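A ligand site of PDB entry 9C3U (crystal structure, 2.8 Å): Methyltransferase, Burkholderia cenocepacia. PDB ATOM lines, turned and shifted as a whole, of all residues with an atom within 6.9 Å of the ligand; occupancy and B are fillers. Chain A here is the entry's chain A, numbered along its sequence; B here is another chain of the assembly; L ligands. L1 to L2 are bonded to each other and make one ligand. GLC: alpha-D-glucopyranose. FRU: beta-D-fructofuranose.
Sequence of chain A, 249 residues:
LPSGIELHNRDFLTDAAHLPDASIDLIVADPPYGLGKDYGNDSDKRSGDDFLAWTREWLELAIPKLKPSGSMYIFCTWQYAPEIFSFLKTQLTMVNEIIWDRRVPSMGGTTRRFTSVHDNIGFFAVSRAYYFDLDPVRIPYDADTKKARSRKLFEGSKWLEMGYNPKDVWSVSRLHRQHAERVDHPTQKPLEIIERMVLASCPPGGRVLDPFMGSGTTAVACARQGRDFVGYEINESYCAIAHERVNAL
N of Met 94 of chain B sits at hydrogen-bond distance from O6 of FRU L2 (2.7 Å).
O of Gln 79 is in hydrogen-bond range of O1 of FRU L2.
O4 of FRU L2 sits close to OE1 of Gln 79 (3.5 Å).
O1 of FRU L2 lies within hydrogen-bond range of NZ of Lys 89 of chain B (3.2 Å).
The side-chain carboxylate of Glu 83 lies within hydrogen-bond range of an oxygen (O1) of FRU L2, 3.3 Å away.
The side-chain amino group (NZ) of Lys 89 of chain B is in hydrogen-bond range of the backbone carbonyl oxygen (O) of Gln 79 (2.7 Å).
N of Gln 79 sits close to OG1 of Thr 77 (3.4 Å).
NZ of Lys 89 of chain B is in salt-bridge range of OE2 of Glu 83, 2.7 Å away.
N of Gly 48 is in hydrogen-bond range of OH of Tyr 80 (2.8 Å).
Gly 48 touches the ligand.
CZ3 of Trp 78 touches O4 of FRU L2, 3.7 Å away.
CE1 of Tyr 80 touches C1 of FRU L2 (3.5 Å).
C of Thr 93 of chain B touches O6 of FRU L2, 3.6 Å away.
Hydrophobic or aromatic side chains that line the ligand: Trp 78, Tyr 80 and Met 94 of chain B.
Within 4 Å of the ligand: Gly 48, Trp 78, Gln 79, Tyr 80, Glu 83, Lys 89 of chain B, Thr 93 of chain B and Met 94 of chain B.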
ATOM      1  N   GLY A  34     -16.801  23.239   9.574  1.00  0.00           N
ATOM      2  CA  GLY A  34     -17.808  22.503  10.306  1.00  0.00           C
ATOM      3  C   GLY A  34     -18.695  21.662   9.410  1.00  0.00           C
ATOM      4  O   GLY A  34     -19.903  21.558   9.654  1.00  0.00           O
ATOM      5  N   SER A  47     -20.103  20.923  14.949  1.00  0.00           N
ATOM      6  CA  SER A  47     -21.271  21.476  14.295  1.00  0.00           C
ATOM      7  C   SER A  47     -22.082  22.307  15.270  1.00  0.00           C
ATOM      8  O   SER A  47     -22.043  22.090  16.480  1.00  0.00           O
ATOM      9  CB  SER A  47     -22.150  20.368  13.700  1.00  0.00           C
ATOM     10  OG  SER A  47     -22.359  19.327  14.642  1.00  0.00           O
ATOM     11  N   GLY A  48     -22.807  23.284  14.722  1.00  0.00           N
ATOM     12  CA  GLY A  48     -23.724  24.073  15.534  1.00  0.00           C
ATOM     13  C   GLY A  48     -22.997  24.991  16.492  1.00  0.00           C
ATOM     14  O   GLY A  48     -21.954  25.578  16.189  1.00  0.00           O
ATOM     15  N   ASP A  49     -23.574  25.120  17.694  1.00  0.00           N
ATOM     16  CA  ASP A  49     -23.007  26.027  18.690  1.00  0.00           C
ATOM     17  C   ASP A  49     -21.646  25.553  19.183  1.00  0.00           C
ATOM     18  O   ASP A  49     -20.823  26.368  19.587  1.00  0.00           O
ATOM     19  CB  ASP A  49     -23.988  26.198  19.851  1.00  0.00           C
ATOM     20  CG  ASP A  49     -25.307  26.793  19.405  1.00  0.00           C
ATOM     21  OD1 ASP A  49     -25.339  27.488  18.366  1.00  0.00           O
ATOM     22  OD2 ASP A  49     -26.326  26.576  20.106  1.00  0.00           O
ATOM     23  N   LEU A  52     -19.383  26.961  16.605  1.00  0.00           N
ATOM     24  CA  LEU A  52     -19.313  28.415  16.748  1.00  0.00           C
ATOM     25  C   LEU A  52     -18.468  28.815  17.939  1.00  0.00           C
ATOM     26  O   LEU A  52     -17.682  29.770  17.874  1.00  0.00           O
ATOM     27  CB  LEU A  52     -20.726  28.988  16.851  1.00  0.00           C
ATOM     28  CG  LEU A  52     -21.283  29.597  15.562  1.00  0.00           C
ATOM     29  CD1 LEU A  52     -20.919  28.737  14.363  1.00  0.00           C
ATOM     30  CD2 LEU A  52     -22.782  29.792  15.653  1.00  0.00           C
ATOM     31  N   THR A  77     -18.551  28.682   5.305  1.00  0.00           N
ATOM     32  CA  THR A  77     -19.734  28.314   4.543  1.00  0.00           C
ATOM     33  C   THR A  77     -20.897  29.208   4.939  1.00  0.00           C
ATOM     34  O   THR A  77     -20.922  29.793   6.024  1.00  0.00           O
ATOM     35  CB  THR A  77     -20.102  26.851   4.773  1.00  0.00           C
ATOM     36  OG1 THR A  77     -21.340  26.564   4.116  1.00  0.00           O
ATOM     37  CG2 THR A  77     -20.226  26.555   6.255  1.00  0.00           C
ATOM     38  N   TRP A  78     -21.866  29.318   4.029  1.00  0.00           N
ATOM     39  CA  TRP A  78     -23.051  30.117   4.304  1.00  0.00           C
ATOM     40  C   TRP A  78     -23.817  29.592   5.519  1.00  0.00           C
ATOM     41  O   TRP A  78     -24.534  30.357   6.173  1.00  0.00           O
ATOM     42  CB  TRP A  78     -23.972  30.126   3.080  1.00  0.00           C
ATOM     43  CG  TRP A  78     -24.471  28.754   2.735  1.00  0.00           C
ATOM     44  CD1 TRP A  78     -23.889  27.843   1.893  1.00  0.00           C
ATOM     45  CD2 TRP A  78     -25.649  28.118   3.249  1.00  0.00           C
ATOM     46  NE1 TRP A  78     -24.632  26.701   1.850  1.00  0.00           N
ATOM     47  CE2 TRP A  78     -25.716  26.837   2.670  1.00  0.00           C
ATOM     48  CE3 TRP A  78     -26.648  28.513   4.148  1.00  0.00           C
ATOM     49  CZ2 TRP A  78     -26.753  25.946   2.956  1.00  0.00           C
ATOM     50  CZ3 TRP A  78     -27.675  27.631   4.424  1.00  0.00           C
ATOM     51  CH2 TRP A  78     -27.721  26.361   3.837  1.00  0.00           C
ATOM     52  N   GLN A  79     -23.655  28.310   5.833  1.00  0.00           N
ATOM     53  CA  GLN A  79     -24.375  27.702   6.940  1.00  0.00           C
ATOM     54  C   GLN A  79     -23.989  28.309   8.284  1.00  0.00           C
ATOM     55  O   GLN A  79     -24.784  28.262   9.221  1.00  0.00           O
ATOM     56  CB  GLN A  79     -24.127  26.194   6.967  1.00  0.00           C
ATOM     57  CG  GLN A  79     -24.008  25.580   5.585  1.00  0.00           C
ATOM     58  CD  GLN A  79     -24.223  24.072   5.598  1.00  0.00           C
ATOM     59  OE1 GLN A  79     -24.986  23.555   6.423  1.00  0.00           O
ATOM     60  NE2 GLN A  79     -23.563  23.374   4.696  1.00  0.00           N
ATOM     61  N   TYR A  80     -22.795  28.879   8.387  1.00  0.00           N
ATOM     62  CA  TYR A  80     -22.350  29.517   9.612  1.00  0.00           C
ATOM     63  C   TYR A  80     -21.927  30.967   9.429  1.00  0.00           C
ATOM     64  O   TYR A  80     -21.717  31.665  10.429  1.00  0.00           O
ATOM     65  CB  TYR A  80     -21.176  28.729  10.234  1.00  0.00           C
ATOM     66  CG  TYR A  80     -21.561  27.341  10.696  1.00  0.00           C
ATOM     67  CD1 TYR A  80     -22.484  27.163  11.715  1.00  0.00           C
ATOM     68  CD2 TYR A  80     -20.993  26.213  10.117  1.00  0.00           C
ATOM     69  CE1 TYR A  80     -22.833  25.897  12.148  1.00  0.00           C
ATOM     70  CE2 TYR A  80     -21.340  24.945  10.540  1.00  0.00           C
ATOM     71  CZ  TYR A  80     -22.255  24.788  11.557  1.00  0.00           C
ATOM     72  OH  TYR A  80     -22.606  23.531  11.988  1.00  0.00           O
ATOM     73  N   ALA A  81     -21.838  31.441   8.183  1.00  0.00           N
ATOM     74  CA  ALA A  81     -21.286  32.774   7.919  1.00  0.00           C
ATOM     75  C   ALA A  81     -22.024  33.902   8.626  1.00  0.00           C
ATOM     76  O   ALA A  81     -21.346  34.787   9.181  1.00  0.00           O
ATOM     77  CB  ALA A  81     -21.239  33.011   6.410  1.00  0.00           C
ATOM     78  N   GLU A  83     -23.425  34.062  11.528  1.00  0.00           N
ATOM     79  CA  GLU A  83     -23.095  34.123  12.956  1.00  0.00           C
ATOM     80  C   GLU A  83     -21.629  34.495  13.165  1.00  0.00           C
ATOM     81  O   GLU A  83     -21.313  35.353  14.008  1.00  0.00           O
ATOM     82  CB  GLU A  83     -23.420  32.796  13.639  1.00  0.00           C
ATOM     83  CG  GLU A  83     -24.873  32.375  13.517  1.00  0.00           C
ATOM     84  CD  GLU A  83     -25.176  31.655  12.217  1.00  0.00           C
ATOM     85  OE1 GLU A  83     -25.035  32.282  11.149  1.00  0.00           O
ATOM     86  OE2 GLU A  83     -25.555  30.465  12.259  1.00  0.00           O
ATOM     87  N   ARG A 113     -33.007  21.841  -3.060  1.00  0.00           N
ATOM     88  CA  ARG A 113     -32.332  23.103  -2.829  1.00  0.00           C
ATOM     89  C   ARG A 113     -31.357  23.352  -3.967  1.00  0.00           C
ATOM     90  O   ARG A 113     -31.027  22.439  -4.732  1.00  0.00           O
ATOM     91  CB  ARG A 113     -31.592  23.102  -1.482  1.00  0.00           C
ATOM     92  CG  ARG A 113     -30.100  22.780  -1.579  1.00  0.00           C
ATOM     93  CD  ARG A 113     -29.562  22.168  -0.293  1.00  0.00           C
ATOM     94  NE  ARG A 113     -29.790  22.988   0.883  1.00  0.00           N
ATOM     95  CZ  ARG A 113     -30.345  22.539   2.005  1.00  0.00           C
ATOM     96  NH1 ARG A 113     -30.760  21.292   2.125  1.00  0.00           N
ATOM     97  NH2 ARG A 113     -30.484  23.375   3.030  1.00  0.00           N
ATOM     98  N   LYS B  89     -32.647  32.821  11.316  1.00  0.00           N
ATOM     99  CA  LYS B  89     -32.386  31.423  11.657  1.00  0.00           C
ATOM    100  C   LYS B  89     -32.993  31.031  12.996  1.00  0.00           C
ATOM    101  O   LYS B  89     -33.206  29.841  13.245  1.00  0.00           O
ATOM    102  CB  LYS B  89     -30.875  31.160  11.667  1.00  0.00           C
ATOM    103  CG  LYS B  89     -30.268  31.082  10.273  1.00  0.00           C
ATOM    104  CD  LYS B  89     -28.771  31.282  10.316  1.00  0.00           C
ATOM    105  CE  LYS B  89     -28.042  29.955  10.363  1.00  0.00           C
ATOM    106  NZ  LYS B  89     -26.656  30.072   9.832  1.00  0.00           N
ATOM    107  N   LEU B  92     -37.042  30.734  11.340  1.00  0.00           N
ATOM    108  CA  LEU B  92     -37.185  29.711  10.289  1.00  0.00           C
ATOM    109  C   LEU B  92     -35.838  29.024  10.090  1.00  0.00           C
ATOM    110  O   LEU B  92     -34.869  29.466  10.714  1.00  0.00           O
ATOM    111  CB  LEU B  92     -37.607  30.494   9.046  1.00  0.00           C
ATOM    112  CG  LEU B  92     -39.092  30.528   8.682  1.00  0.00           C
ATOM    113  CD1 LEU B  92     -40.013  30.603   9.889  1.00  0.00           C
ATOM    114  CD2 LEU B  92     -39.357  31.675   7.743  1.00  0.00           C
ATOM    115  N   THR B  93     -35.785  27.988   9.266  1.00  0.00           N
ATOM    116  CA  THR B  93     -34.556  27.295   8.936  1.00  0.00           C
ATOM    117  C   THR B  93     -34.025  27.814   7.605  1.00  0.00           C
ATOM    118  O   THR B  93     -34.790  28.036   6.666  1.00  0.00           O
ATOM    119  CB  THR B  93     -34.770  25.783   8.846  1.00  0.00           C
ATOM    120  OG1 THR B  93     -35.297  25.459   7.544  1.00  0.00           O
ATOM    121  CG2 THR B  93     -35.756  25.328   9.910  1.00  0.00           C
ATOM    122  N   MET B  94     -32.705  28.028   7.541  1.00  0.00           N
ATOM    123  CA  MET B  94     -32.086  28.476   6.298  1.00  0.00           C
ATOM    124  C   MET B  94     -31.863  27.290   5.368  1.00  0.00           C
ATOM    125  O   MET B  94     -31.106  26.378   5.699  1.00  0.00           O
ATOM    126  CB  MET B  94     -30.766  29.189   6.578  1.00  0.00           C
ATOM    127  CG  MET B  94     -30.572  30.438   5.735  1.00  0.00           C
ATOM    128  SD  MET B  94     -29.066  31.351   6.098  1.00  0.00           S
ATOM    129  CE  MET B  94     -28.765  32.111   4.515  1.00  0.00           C
ATOM    130  N   VAL B  95     -32.532  27.318   4.220  1.00  0.00           N
ATOM    131  CA  VAL B  95     -32.291  26.301   3.205  1.00  0.00           C
ATOM    132  C   VAL B  95     -31.105  26.695   2.337  1.00  0.00           C
ATOM    133  O   VAL B  95     -30.269  25.854   1.989  1.00  0.00           O
ATOM    134  CB  VAL B  95     -33.564  26.060   2.373  1.00  0.00           C
ATOM    135  CG1 VAL B  95     -33.275  25.056   1.261  1.00  0.00           C
ATOM    136  CG2 VAL B  95     -34.695  25.572   3.253  1.00  0.00           C
ATOM    137  N   PHE B 124     -35.170  30.859   3.229  1.00  0.00           N
ATOM    138  CA  PHE B 124     -35.613  30.235   4.467  1.00  0.00           C
ATOM    139  C   PHE B 124     -36.911  29.482   4.222  1.00  0.00           C
ATOM    140  O   PHE B 124     -37.637  29.735   3.264  1.00  0.00           O
ATOM    141  CB  PHE B 124     -35.824  31.277   5.568  1.00  0.00           C
ATOM    142  CG  PHE B 124     -34.584  32.045   5.943  1.00  0.00           C
ATOM    143  CD1 PHE B 124     -34.155  33.114   5.172  1.00  0.00           C
ATOM    144  CD2 PHE B 124     -33.866  31.699   7.077  1.00  0.00           C
ATOM    145  CE1 PHE B 124     -33.021  33.819   5.515  1.00  0.00           C
ATOM    146  CE2 PHE B 124     -32.733  32.404   7.420  1.00  0.00           C
ATOM    147  CZ  PHE B 124     -32.300  33.461   6.642  1.00  0.00           C
ATOM    148  N   ARG B 128     -39.506  21.569   7.434  1.00  0.00           N
ATOM    149  CA  ARG B 128     -38.666  20.764   6.555  1.00  0.00           C
ATOM    150  C   ARG B 128     -39.454  20.190   5.383  1.00  0.00           C
ATOM    151  O   ARG B 128     -38.853  19.728   4.416  1.00  0.00           O
ATOM    152  CB  ARG B 128     -38.026  19.632   7.358  1.00  0.00           C
ATOM    153  CG  ARG B 128     -37.839  19.942   8.824  1.00  0.00           C
ATOM    154  CD  ARG B 128     -37.269  18.753   9.560  1.00  0.00           C
ATOM    155  NE  ARG B 128     -36.283  18.046   8.746  1.00  0.00           N
ATOM    156  CZ  ARG B 128     -35.631  16.957   9.133  1.00  0.00           C
ATOM    157  NH1 ARG B 128     -35.823  16.427  10.326  1.00  0.00           N
ATOM    158  NH2 ARG B 128     -34.769  16.393   8.291  1.00  0.00           N
HETATM  159  C1  GLC L   1     -28.223  24.191  13.055  1.00  0.00           C
HETATM  160  C2  GLC L   1     -27.987  22.995  13.976  1.00  0.00           C
HETATM  161  C3  GLC L   1     -28.503  21.719  13.313  1.00  0.00           C
HETATM  162  C4  GLC L   1     -29.935  21.892  12.816  1.00  0.00           C
HETATM  163  C5  GLC L   1     -30.090  23.184  12.029  1.00  0.00           C
HETATM  164  C6  GLC L   1     -31.541  23.431  11.669  1.00  0.00           C
HETATM  165  O2  GLC L   1     -26.609  22.861  14.242  1.00  0.00           O
HETATM  166  O3  GLC L   1     -28.461  20.668  14.253  1.00  0.00           O
HETATM  167  O4  GLC L   1     -30.276  20.798  11.997  1.00  0.00           O
HETATM  168  O5  GLC L   1     -29.611  24.271  12.787  1.00  0.00           O
HETATM  169  O6  GLC L   1     -31.898  22.644  10.549  1.00  0.00           O
HETATM  170  C1  FRU L   2     -26.288  26.058  12.012  1.00  0.00           C
HETATM  171  C2  FRU L   2     -27.238  25.214  11.175  1.00  0.00           C
HETATM  172  C3  FRU L   2     -26.626  24.877   9.827  1.00  0.00           C
HETATM  173  C4  FRU L   2     -27.690  25.240   8.808  1.00  0.00           C
HETATM  174  C5  FRU L   2     -28.657  26.143   9.563  1.00  0.00           C
HETATM  175  C6  FRU L   2     -30.104  25.856   9.183  1.00  0.00           C
HETATM  176  O1  FRU L   2     -26.118  27.318  11.391  1.00  0.00           O
HETATM  177  O2  FRU L   2     -27.500  23.999  11.858  1.00  0.00           O
HETATM  178  O3  FRU L   2     -26.340  23.504   9.749  1.00  0.00           O
HETATM  179  O4  FRU L   2     -27.127  25.948   7.727  1.00  0.00           O
HETATM  180  O5  FRU L   2     -28.442  25.917  10.942  1.00  0.00           O
HETATM  181  O6  FRU L   2     -30.846  27.055   9.213  1.00  0.00           O
